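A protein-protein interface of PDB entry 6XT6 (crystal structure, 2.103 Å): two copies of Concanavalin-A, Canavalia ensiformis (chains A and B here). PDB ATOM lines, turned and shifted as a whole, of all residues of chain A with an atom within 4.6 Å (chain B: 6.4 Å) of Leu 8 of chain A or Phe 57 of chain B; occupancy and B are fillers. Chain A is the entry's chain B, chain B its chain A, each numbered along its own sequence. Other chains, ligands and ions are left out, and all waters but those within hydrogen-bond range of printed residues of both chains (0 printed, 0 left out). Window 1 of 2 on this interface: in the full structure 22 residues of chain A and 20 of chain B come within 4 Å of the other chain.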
ATOM      1  N   ALA A   7      21.953  18.392  -8.190  1.00  0.00           N
ATOM      2  CA  ALA A   7      23.287  18.793  -8.695  1.00  0.00           C
ATOM      3  C   ALA A   7      23.363  18.659 -10.209  1.00  0.00           C
ATOM      4  O   ALA A   7      22.761  17.728 -10.763  1.00  0.00           O
ATOM      5  CB  ALA A   7      24.372  17.998  -8.037  1.00  0.00           C
ATOM      6  N   LEU A   8      24.080  19.592 -10.832  1.00  0.00           N
ATOM      7  CA  LEU A   8      24.536  19.499 -12.235  1.00  0.00           C
ATOM      8  C   LEU A   8      26.045  19.746 -12.278  1.00  0.00           C
ATOM      9  O   LEU A   8      26.498  20.730 -11.644  1.00  0.00           O
ATOM     10  CB  LEU A   8      23.762  20.532 -13.050  1.00  0.00           C
ATOM     11  CG  LEU A   8      24.225  20.702 -14.488  1.00  0.00           C
ATOM     12  CD1 LEU A   8      23.793  19.520 -15.328  1.00  0.00           C
ATOM     13  CD2 LEU A   8      23.657  21.981 -15.056  1.00  0.00           C
ATOM     14  N   HIS A   9      26.780  18.859 -12.953  1.00  0.00           N
ATOM     15  CA  HIS A   9      28.233  18.983 -13.238  1.00  0.00           C
ATOM     16  C   HIS A   9      28.455  18.709 -14.728  1.00  0.00           C
ATOM     17  O   HIS A   9      27.902  17.741 -15.240  1.00  0.00           O
ATOM     18  CB  HIS A   9      29.051  18.091 -12.292  1.00  0.00           C
ATOM     19  CG  HIS A   9      30.500  17.983 -12.620  1.00  0.00           C
ATOM     20  ND1 HIS A   9      31.364  19.052 -12.523  1.00  0.00           N
ATOM     21  CD2 HIS A   9      31.248  16.933 -13.028  1.00  0.00           C
ATOM     22  CE1 HIS A   9      32.583  18.667 -12.863  1.00  0.00           C
ATOM     23  NE2 HIS A   9      32.536  17.371 -13.186  1.00  0.00           N
ATOM     24  N   PHE A  10      29.204  19.565 -15.414  1.00  0.00           N
ATOM     25  CA  PHE A  10      29.748  19.249 -16.750  1.00  0.00           C
ATOM     26  C   PHE A  10      31.220  19.658 -16.772  1.00  0.00           C
ATOM     27  O   PHE A  10      31.650  20.534 -15.985  1.00  0.00           O
ATOM     28  CB  PHE A  10      28.865  19.859 -17.851  1.00  0.00           C
ATOM     29  CG  PHE A  10      28.881  21.365 -17.896  1.00  0.00           C
ATOM     30  CD1 PHE A  10      29.981  22.052 -18.395  1.00  0.00           C
ATOM     31  CD2 PHE A  10      27.800  22.095 -17.445  1.00  0.00           C
ATOM     32  CE1 PHE A  10      29.996  23.440 -18.428  1.00  0.00           C
ATOM     33  CE2 PHE A  10      27.814  23.481 -17.487  1.00  0.00           C
ATOM     34  CZ  PHE A  10      28.909  24.148 -17.970  1.00  0.00           C
ATOM     35  N   PHE A  57      25.801  26.435 -21.833  1.00  0.00           N
ATOM     36  CA  PHE A  57      25.474  25.008 -21.604  1.00  0.00           C
ATOM     37  C   PHE A  57      23.975  24.818 -21.905  1.00  0.00           C
ATOM     38  O   PHE A  57      23.140  25.675 -21.625  1.00  0.00           O
ATOM     39  CB  PHE A  57      25.918  24.529 -20.223  1.00  0.00           C
ATOM     40  CG  PHE A  57      25.829  23.027 -20.100  1.00  0.00           C
ATOM     41  CD1 PHE A  57      26.682  22.203 -20.829  1.00  0.00           C
ATOM     42  CD2 PHE A  57      24.830  22.429 -19.348  1.00  0.00           C
ATOM     43  CE1 PHE A  57      26.560  20.823 -20.763  1.00  0.00           C
ATOM     44  CE2 PHE A  57      24.716  21.045 -19.292  1.00  0.00           C
ATOM     45  CZ  PHE A  57      25.580  20.251 -19.988  1.00  0.00           C
ATOM     46  N   ALA A  59      21.568  22.518 -20.859  1.00  0.00           N
ATOM     47  CA  ALA A  59      20.637  22.288 -19.723  1.00  0.00           C
ATOM     48  C   ALA A  59      20.525  23.575 -18.912  1.00  0.00           C
ATOM     49  O   ALA A  59      21.540  24.118 -18.489  1.00  0.00           O
ATOM     50  CB  ALA A  59      21.088  21.139 -18.851  1.00  0.00           C
ATOM     51  N   PRO A  60      19.304  24.112 -18.690  1.00  0.00           N
ATOM     52  CA  PRO A  60      19.094  25.149 -17.686  1.00  0.00           C
ATOM     53  C   PRO A  60      19.529  24.676 -16.292  1.00  0.00           C
ATOM     54  O   PRO A  60      19.461  23.492 -16.011  1.00  0.00           O
ATOM     55  CB  PRO A  60      17.575  25.363 -17.666  1.00  0.00           C
ATOM     56  CG  PRO A  60      17.097  24.865 -19.006  1.00  0.00           C
ATOM     57  CD  PRO A  60      18.065  23.763 -19.393  1.00  0.00           C
ATOM     58  N   VAL A  61      19.935  25.615 -15.447  1.00  0.00           N
ATOM     59  CA  VAL A  61      20.395  25.349 -14.058  1.00  0.00           C
ATOM     60  C   VAL A  61      19.397  25.993 -13.080  1.00  0.00           C
ATOM     61  O   VAL A  61      19.056  27.181 -13.259  1.00  0.00           O
ATOM     62  CB  VAL A  61      21.825  25.896 -13.896  1.00  0.00           C
ATOM     63  CG1 VAL A  61      22.426  25.574 -12.532  1.00  0.00           C
ATOM     64  CG2 VAL A  61      22.725  25.407 -15.017  1.00  0.00           C
ATOM     65  N   PHE A 245      31.820  23.164 -14.761  1.00  0.00           N
ATOM     66  CA  PHE A 245      30.745  23.811 -13.970  1.00  0.00           C
ATOM     67  C   PHE A 245      30.152  22.755 -13.047  1.00  0.00           C
ATOM     68  O   PHE A 245      29.926  21.630 -13.507  1.00  0.00           O
ATOM     69  CB  PHE A 245      29.670  24.429 -14.876  1.00  0.00           C
ATOM     70  CG  PHE A 245      28.577  25.138 -14.113  1.00  0.00           C
ATOM     71  CD1 PHE A 245      28.769  26.426 -13.628  1.00  0.00           C
ATOM     72  CD2 PHE A 245      27.382  24.492 -13.834  1.00  0.00           C
ATOM     73  CE1 PHE A 245      27.784  27.040 -12.872  1.00  0.00           C
ATOM     74  CE2 PHE A 245      26.408  25.111 -13.075  1.00  0.00           C
ATOM     75  CZ  PHE A 245      26.609  26.381 -12.599  1.00  0.00           C
ATOM     76  N   THR A 246      29.972  23.105 -11.776  1.00  0.00           N
ATOM     77  CA  THR A 246      29.193  22.324 -10.776  1.00  0.00           C
ATOM     78  C   THR A 246      28.238  23.255 -10.020  1.00  0.00           C
ATOM     79  O   THR A 246      28.731  24.250  -9.470  1.00  0.00           O
ATOM     80  CB  THR A 246      30.094  21.646  -9.740  1.00  0.00           C
ATOM     81  OG1 THR A 246      31.069  20.873 -10.436  1.00  0.00           O
ATOM     82  CG2 THR A 246      29.310  20.779  -8.776  1.00  0.00           C
ATOM     83  N   SER A 247      26.951  22.924  -9.982  1.00  0.00           N
ATOM     84  CA  SER A 247      25.901  23.613  -9.184  1.00  0.00           C
ATOM     85  C   SER A 247      25.210  22.601  -8.252  1.00  0.00           C
ATOM     86  O   SER A 247      24.838  21.487  -8.738  1.00  0.00           O
ATOM     87  CB  SER A 247      24.914  24.292 -10.094  1.00  0.00           C
ATOM     88  OG  SER A 247      24.086  25.196  -9.373  1.00  0.00           O
ATOM     89  N   LEU B   8      29.521  14.515 -17.975  1.00  0.00           N
ATOM     90  CA  LEU B   8      28.201  15.013 -17.530  1.00  0.00           C
ATOM     91  C   LEU B   8      27.817  14.266 -16.267  1.00  0.00           C
ATOM     92  O   LEU B   8      27.915  13.011 -16.251  1.00  0.00           O
ATOM     93  CB  LEU B   8      27.132  14.781 -18.603  1.00  0.00           C
ATOM     94  CG  LEU B   8      25.737  15.285 -18.245  1.00  0.00           C
ATOM     95  CD1 LEU B   8      25.725  16.793 -18.092  1.00  0.00           C
ATOM     96  CD2 LEU B   8      24.723  14.851 -19.283  1.00  0.00           C
ATOM     97  N   HIS B   9      27.331  15.003 -15.284  1.00  0.00           N
ATOM     98  CA  HIS B   9      26.714  14.405 -14.081  1.00  0.00           C
ATOM     99  C   HIS B   9      25.465  15.203 -13.694  1.00  0.00           C
ATOM    100  O   HIS B   9      25.518  16.451 -13.638  1.00  0.00           O
ATOM    101  CB  HIS B   9      27.751  14.316 -12.958  1.00  0.00           C
ATOM    102  CG  HIS B   9      27.123  14.055 -11.638  1.00  0.00           C
ATOM    103  ND1 HIS B   9      26.632  12.812 -11.299  1.00  0.00           N
ATOM    104  CD2 HIS B   9      26.827  14.886 -10.615  1.00  0.00           C
ATOM    105  CE1 HIS B   9      26.108  12.869 -10.086  1.00  0.00           C
ATOM    106  NE2 HIS B   9      26.213  14.136  -9.649  1.00  0.00           N
ATOM    107  N   PHE B  10      24.372  14.509 -13.435  1.00  0.00           N
ATOM    108  CA  PHE B  10      23.202  15.129 -12.780  1.00  0.00           C
ATOM    109  C   PHE B  10      22.701  14.241 -11.649  1.00  0.00           C
ATOM    110  O   PHE B  10      22.941  13.009 -11.596  1.00  0.00           O
ATOM    111  CB  PHE B  10      22.144  15.504 -13.806  1.00  0.00           C
ATOM    112  CG  PHE B  10      21.532  14.366 -14.573  1.00  0.00           C
ATOM    113  CD1 PHE B  10      20.631  13.507 -13.968  1.00  0.00           C
ATOM    114  CD2 PHE B  10      21.796  14.202 -15.924  1.00  0.00           C
ATOM    115  CE1 PHE B  10      20.006  12.509 -14.703  1.00  0.00           C
ATOM    116  CE2 PHE B  10      21.200  13.181 -16.645  1.00  0.00           C
ATOM    117  CZ  PHE B  10      20.289  12.351 -16.040  1.00  0.00           C
ATOM    118  N   MET B  11      22.022  14.900 -10.722  1.00  0.00           N
ATOM    119  CA  MET B  11      21.381  14.270  -9.549  1.00  0.00           C
ATOM    120  C   MET B  11      20.089  15.024  -9.217  1.00  0.00           C
ATOM    121  O   MET B  11      20.144  16.237  -8.941  1.00  0.00           O
ATOM    122  CB  MET B  11      22.339  14.304  -8.363  1.00  0.00           C
ATOM    123  CG  MET B  11      21.852  13.493  -7.181  1.00  0.00           C
ATOM    124  SD  MET B  11      23.212  13.200  -6.031  1.00  0.00           S
ATOM    125  CE  MET B  11      23.623  14.865  -5.506  1.00  0.00           C
ATOM    126  N   PHE B  12      18.962  14.318  -9.301  1.00  0.00           N
ATOM    127  CA  PHE B  12      17.638  14.699  -8.747  1.00  0.00           C
ATOM    128  C   PHE B  12      17.405  13.901  -7.463  1.00  0.00           C
ATOM    129  O   PHE B  12      17.294  12.670  -7.550  1.00  0.00           O
ATOM    130  CB  PHE B  12      16.533  14.412  -9.766  1.00  0.00           C
ATOM    131  CG  PHE B  12      16.704  15.079 -11.109  1.00  0.00           C
ATOM    132  CD1 PHE B  12      16.251  16.370 -11.329  1.00  0.00           C
ATOM    133  CD2 PHE B  12      17.285  14.405 -12.170  1.00  0.00           C
ATOM    134  CE1 PHE B  12      16.382  16.967 -12.570  1.00  0.00           C
ATOM    135  CE2 PHE B  12      17.413  15.007 -13.411  1.00  0.00           C
ATOM    136  CZ  PHE B  12      16.968  16.289 -13.606  1.00  0.00           C
ATOM    137  N   ASP B  21      14.980  21.176 -16.642  1.00  0.00           N
ATOM    138  CA  ASP B  21      16.065  20.276 -17.115  1.00  0.00           C
ATOM    139  C   ASP B  21      15.526  18.855 -17.363  1.00  0.00           C
ATOM    140  O   ASP B  21      16.344  17.963 -17.539  1.00  0.00           O
ATOM    141  CB  ASP B  21      17.261  20.296 -16.157  1.00  0.00           C
ATOM    142  CG  ASP B  21      16.909  20.060 -14.708  1.00  0.00           C
ATOM    143  OD1 ASP B  21      15.709  19.800 -14.450  1.00  0.00           O
ATOM    144  OD2 ASP B  21      17.825  20.195 -13.844  1.00  0.00           O
ATOM    145  N   LEU B  22      14.209  18.645 -17.432  1.00  0.00           N
ATOM    146  CA  LEU B  22      13.616  17.344 -17.836  1.00  0.00           C
ATOM    147  C   LEU B  22      12.649  17.569 -18.987  1.00  0.00           C
ATOM    148  O   LEU B  22      11.892  18.527 -18.919  1.00  0.00           O
ATOM    149  CB  LEU B  22      12.854  16.724 -16.662  1.00  0.00           C
ATOM    150  CG  LEU B  22      13.700  16.167 -15.524  1.00  0.00           C
ATOM    151  CD1 LEU B  22      12.806  15.450 -14.525  1.00  0.00           C
ATOM    152  CD2 LEU B  22      14.790  15.228 -16.042  1.00  0.00           C
ATOM    153  N   ILE B  23      12.662  16.688 -19.979  1.00  0.00           N
ATOM    154  CA  ILE B  23      11.602  16.589 -21.031  1.00  0.00           C
ATOM    155  C   ILE B  23      10.605  15.511 -20.581  1.00  0.00           C
ATOM    156  O   ILE B  23      10.989  14.317 -20.567  1.00  0.00           O
ATOM    157  CB  ILE B  23      12.219  16.246 -22.401  1.00  0.00           C
ATOM    158  CG1 ILE B  23      13.286  17.257 -22.825  1.00  0.00           C
ATOM    159  CG2 ILE B  23      11.132  16.082 -23.456  1.00  0.00           C
ATOM    160  CD1 ILE B  23      14.142  16.799 -23.996  1.00  0.00           C
ATOM    161  N   ALA B  55      10.701  10.545 -18.763  1.00  0.00           N
ATOM    162  CA  ALA B  55      11.476  11.748 -18.426  1.00  0.00           C
ATOM    163  C   ALA B  55      12.846  11.613 -19.092  1.00  0.00           C
ATOM    164  O   ALA B  55      13.552  10.580 -18.855  1.00  0.00           O
ATOM    165  CB  ALA B  55      11.586  11.880 -16.925  1.00  0.00           C
ATOM    166  N   LEU B  56      13.184  12.581 -19.931  1.00  0.00           N
ATOM    167  CA  LEU B  56      14.538  12.668 -20.539  1.00  0.00           C
ATOM    168  C   LEU B  56      15.262  13.891 -19.977  1.00  0.00           C
ATOM    169  O   LEU B  56      14.616  14.955 -19.828  1.00  0.00           O
ATOM    170  CB  LEU B  56      14.400  12.705 -22.061  1.00  0.00           C
ATOM    171  CG  LEU B  56      13.785  11.438 -22.646  1.00  0.00           C
ATOM    172  CD1 LEU B  56      12.265  11.534 -22.637  1.00  0.00           C
ATOM    173  CD2 LEU B  56      14.299  11.183 -24.051  1.00  0.00           C
ATOM    174  N   PHE B  57      16.531  13.720 -19.618  1.00  0.00           N
ATOM    175  CA  PHE B  57      17.425  14.854 -19.287  1.00  0.00           C
ATOM    176  C   PHE B  57      17.563  15.728 -20.529  1.00  0.00           C
ATOM    177  O   PHE B  57      17.752  15.183 -21.637  1.00  0.00           O
ATOM    178  CB  PHE B  57      18.797  14.395 -18.818  1.00  0.00           C
ATOM    179  CG  PHE B  57      19.588  15.496 -18.174  1.00  0.00           C
ATOM    180  CD1 PHE B  57      19.142  16.078 -17.003  1.00  0.00           C
ATOM    181  CD2 PHE B  57      20.775  15.945 -18.732  1.00  0.00           C
ATOM    182  CE1 PHE B  57      19.871  17.084 -16.390  1.00  0.00           C
ATOM    183  CE2 PHE B  57      21.508  16.947 -18.114  1.00  0.00           C
ATOM    184  CZ  PHE B  57      21.055  17.515 -16.946  1.00  0.00           C
ATOM    185  N   TYR B  58      17.448  17.044 -20.340  1.00  0.00           N
ATOM    186  CA  TYR B  58      17.307  18.033 -21.436  1.00  0.00           C
ATOM    187  C   TYR B  58      18.571  18.009 -22.306  1.00  0.00           C
ATOM    188  O   TYR B  58      18.485  18.158 -23.544  1.00  0.00           O
ATOM    189  CB  TYR B  58      16.962  19.399 -20.833  1.00  0.00           C
ATOM    190  CG  TYR B  58      16.546  20.445 -21.840  1.00  0.00           C
ATOM    191  CD1 TYR B  58      15.386  20.307 -22.590  1.00  0.00           C
ATOM    192  CD2 TYR B  58      17.315  21.580 -22.052  1.00  0.00           C
ATOM    193  CE1 TYR B  58      14.998  21.266 -23.518  1.00  0.00           C
ATOM    194  CE2 TYR B  58      16.938  22.552 -22.967  1.00  0.00           C
ATOM    195  CZ  TYR B  58      15.781  22.393 -23.707  1.00  0.00           C
ATOM    196  OH  TYR B  58      15.432  23.343 -24.611  1.00  0.00           O
ATOM    197  N   ALA B  59      19.729  17.822 -21.673  1.00  0.00           N
ATOM    198  CA  ALA B  59      21.053  17.898 -22.330  1.00  0.00           C
ATOM    199  C   ALA B  59      21.375  16.578 -23.025  1.00  0.00           C
ATOM    200  O   ALA B  59      21.318  15.515 -22.407  1.00  0.00           O
ATOM    201  CB  ALA B  59      22.128  18.238 -21.322  1.00  0.00           C
ATOM    202  N   PRO B  60      21.790  16.614 -24.311  1.00  0.00           N
ATOM    203  CA  PRO B  60      22.329  15.426 -24.965  1.00  0.00           C
ATOM    204  C   PRO B  60      23.710  15.020 -24.425  1.00  0.00           C
ATOM    205  O   PRO B  60      24.469  15.872 -23.919  1.00  0.00           O
ATOM    206  CB  PRO B  60      22.398  15.799 -26.446  1.00  0.00           C
ATOM    207  CG  PRO B  60      22.413  17.316 -26.481  1.00  0.00           C
ATOM    208  CD  PRO B  60      21.785  17.795 -25.191  1.00  0.00           C
ATOM    209  N   VAL B  61      23.971  13.716 -24.508  1.00  0.00           N
ATOM    210  CA  VAL B  61      25.152  13.022 -23.926  1.00  0.00           C
ATOM    211  C   VAL B  61      25.980  12.523 -25.104  1.00  0.00           C
ATOM    212  O   VAL B  61      25.377  11.951 -26.035  1.00  0.00           O
ATOM    213  CB  VAL B  61      24.711  11.873 -23.000  1.00  0.00           C
ATOM    214  CG1 VAL B  61      25.874  11.238 -22.290  1.00  0.00           C
ATOM    215  CG2 VAL B  61      23.675  12.343 -21.994  1.00  0.00           C
ATOM    216  N   ARG B 224      20.009  10.973 -25.846  1.00  0.00           N
ATOM    217  CA  ARG B 224      19.393  11.373 -24.554  1.00  0.00           C
ATOM    218  C   ARG B 224      19.236  10.121 -23.699  1.00  0.00           C
ATOM    219  O   ARG B 224      19.051   9.002 -24.241  1.00  0.00           O
ATOM    220  CB  ARG B 224      18.087  12.142 -24.752  1.00  0.00           C
ATOM    221  CG  ARG B 224      18.305  13.607 -25.102  1.00  0.00           C
ATOM    222  CD  ARG B 224      17.084  14.458 -24.902  1.00  0.00           C
ATOM    223  NE  ARG B 224      17.367  15.874 -25.063  1.00  0.00           N
ATOM    224  CZ  ARG B 224      17.084  16.613 -26.137  1.00  0.00           C
ATOM    225  NH1 ARG B 224      16.513  16.081 -27.208  1.00  0.00           N
ATOM    226  NH2 ARG B 224      17.391  17.901 -26.132  1.00  0.00           N
ATOM    227  N   VAL B 225      19.334  10.332 -22.398  1.00  0.00           N
ATOM    228  CA  VAL B 225      19.096   9.296 -21.372  1.00  0.00           C
ATOM    229  C   VAL B 225      17.778   9.642 -20.696  1.00  0.00           C
ATOM    230  O   VAL B 225      17.436  10.839 -20.631  1.00  0.00           O
ATOM    231  CB  VAL B 225      20.268   9.188 -20.378  1.00  0.00           C
ATOM    232  CG1 VAL B 225      21.542   8.791 -21.106  1.00  0.00           C
ATOM    233  CG2 VAL B 225      20.472  10.455 -19.572  1.00  0.00           C
ATOM    234  N   GLY B 226      17.074   8.613 -20.241  1.00  0.00           N
ATOM    235  CA  GLY B 226      15.724   8.782 -19.704  1.00  0.00           C
ATOM    236  C   GLY B 226      15.271   7.608 -18.871  1.00  0.00           C
ATOM    237  O   GLY B 226      15.966   6.560 -18.827  1.00  0.00           O
ATOM    238  N   TRP B 243      17.139  10.149  -9.039  1.00  0.00           N
ATOM    239  CA  TRP B 243      17.750   9.738 -10.317  1.00  0.00           C
ATOM    240  C   TRP B 243      19.041  10.518 -10.510  1.00  0.00           C
ATOM    241  O   TRP B 243      18.994  11.760 -10.564  1.00  0.00           O
ATOM    242  CB  TRP B 243      16.777   9.967 -11.468  1.00  0.00           C
ATOM    243  CG  TRP B 243      17.305   9.594 -12.815  1.00  0.00           C
ATOM    244  CD1 TRP B 243      18.183   8.597 -13.127  1.00  0.00           C
ATOM    245  CD2 TRP B 243      16.929  10.204 -14.057  1.00  0.00           C
ATOM    246  NE1 TRP B 243      18.380   8.552 -14.482  1.00  0.00           N
ATOM    247  CE2 TRP B 243      17.623   9.524 -15.075  1.00  0.00           C
ATOM    248  CE3 TRP B 243      16.085  11.267 -14.400  1.00  0.00           C
ATOM    249  CZ2 TRP B 243      17.490   9.877 -16.419  1.00  0.00           C
ATOM    250  CZ3 TRP B 243      15.955  11.611 -15.724  1.00  0.00           C
ATOM    251  CH2 TRP B 243      16.652  10.926 -16.715  1.00  0.00           C
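The backbone NH (N) of His 9 of chain B lies within hydrogen-bond range of the backbone carbonyl oxygen (O) of His 9 of chain A (2.8 Å). O of Met 11 of chain B lies within hydrogen-bond range of N of Ala 7 of chain A (2.9 Å).
Of the 11 printed residues of chain A, 6 touch a printed residue of chain B. Hydrophobic or aromatic side chains of chain A within 4 Å of the printed part of chain B: Leu 8, Phe 57, Ala 59 and Pro 60. Among the printed residues, no Asp or Glu carboxylate lies within 4 Å of a Lys or Arg side-chain nitrogen of the other chain.
The backbone carbonyl oxygen of Val 225 of chain B is in hydrogen-bond range of the backbone NH of Phe 57 of chain B (3.2 Å). The backbone carbonyl oxygen (O) of Phe 245 of chain A is in hydrogen-bond range of a ring nitrogen (ND1) of His 9 of chain A, at 3.1 Å. O of Leu 8 of chain A is in hydrogen-bond range of N of Ser 247 of chain A, 2.8 Å away. The backbone carbonyl oxygen of Asp 21 of chain B is in hydrogen-bond range of the backbone NH of Tyr 58 of chain B. The side-chain hydroxyl (OG1) of Thr 246 of chain A lies within hydrogen-bond range of a ring nitrogen (ND1) of His 9 of chain A (2.8 Å). The backbone carbonyl oxygen (O) of Tyr 58 of chain B is in hydrogen-bond range of the guanidinium group (NH2) of Arg 224 of chain B.
Leu 8 of chain A touches just these residues of chain B: His 9 (3.5 Å) and Phe 57 (3.8 Å). Phe 57 of chain B touches just one residue of chain A: Leu 8. Of the printed residues of chain A, Tyr 58 of chain B touches Pro 60 (3.5 Å). Of the printed residues of chain B, Pro 60 of chain A touches Asp 21 and Tyr 58. Of the printed residues of chain A, Phe 10 of chain B touches Ala 7 (3.3 Å). Printed residues of chain B within 4 Å of His 9 of chain A: Leu 8 and His 9. Printed residues of chain B within 4 Å of Ala 59 of chain A: Ala 59 (3.95 Å). The nearest residue of chain A that does not touch Phe 57 of chain B is Ala 59 of chain A (4.1 Å). The nearest printed residue of chain A that does not touch Asp 21 of chain B is Ala 59 of chain A (4.8 Å).
Among the printed residues, merely in contact across the chains: Ala 7 of chain A with Phe 10 of chain B, Leu 8 of chain A with His 9 of chain B, Leu 8 of chain A with Phe 57 of chain B, His 9 of chain A with Leu 8 of chain B, Phe 57 of chain A with Leu 8 of chain B, Ala 59 of chain A with Ala 59 of chain B, Pro 60 of chain A with Asp 21 of chain B and Pro 60 of chain A with Tyr 58 of chain B.
Leu 8 of chain A touches His 9 of chain B, and with the chains exchanged His 9 of chain A touches Leu 8 of chain B. Leu 8 of chain A touches Phe 57 of chain B, and with the chains exchanged Phe 57 of chain A touches Leu 8 of chain B. His 9 of chain A touches its own counterpart, His 9 of chain B. Ala 59 of chain A touches its own counterpart, Ala 59 of chain B.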
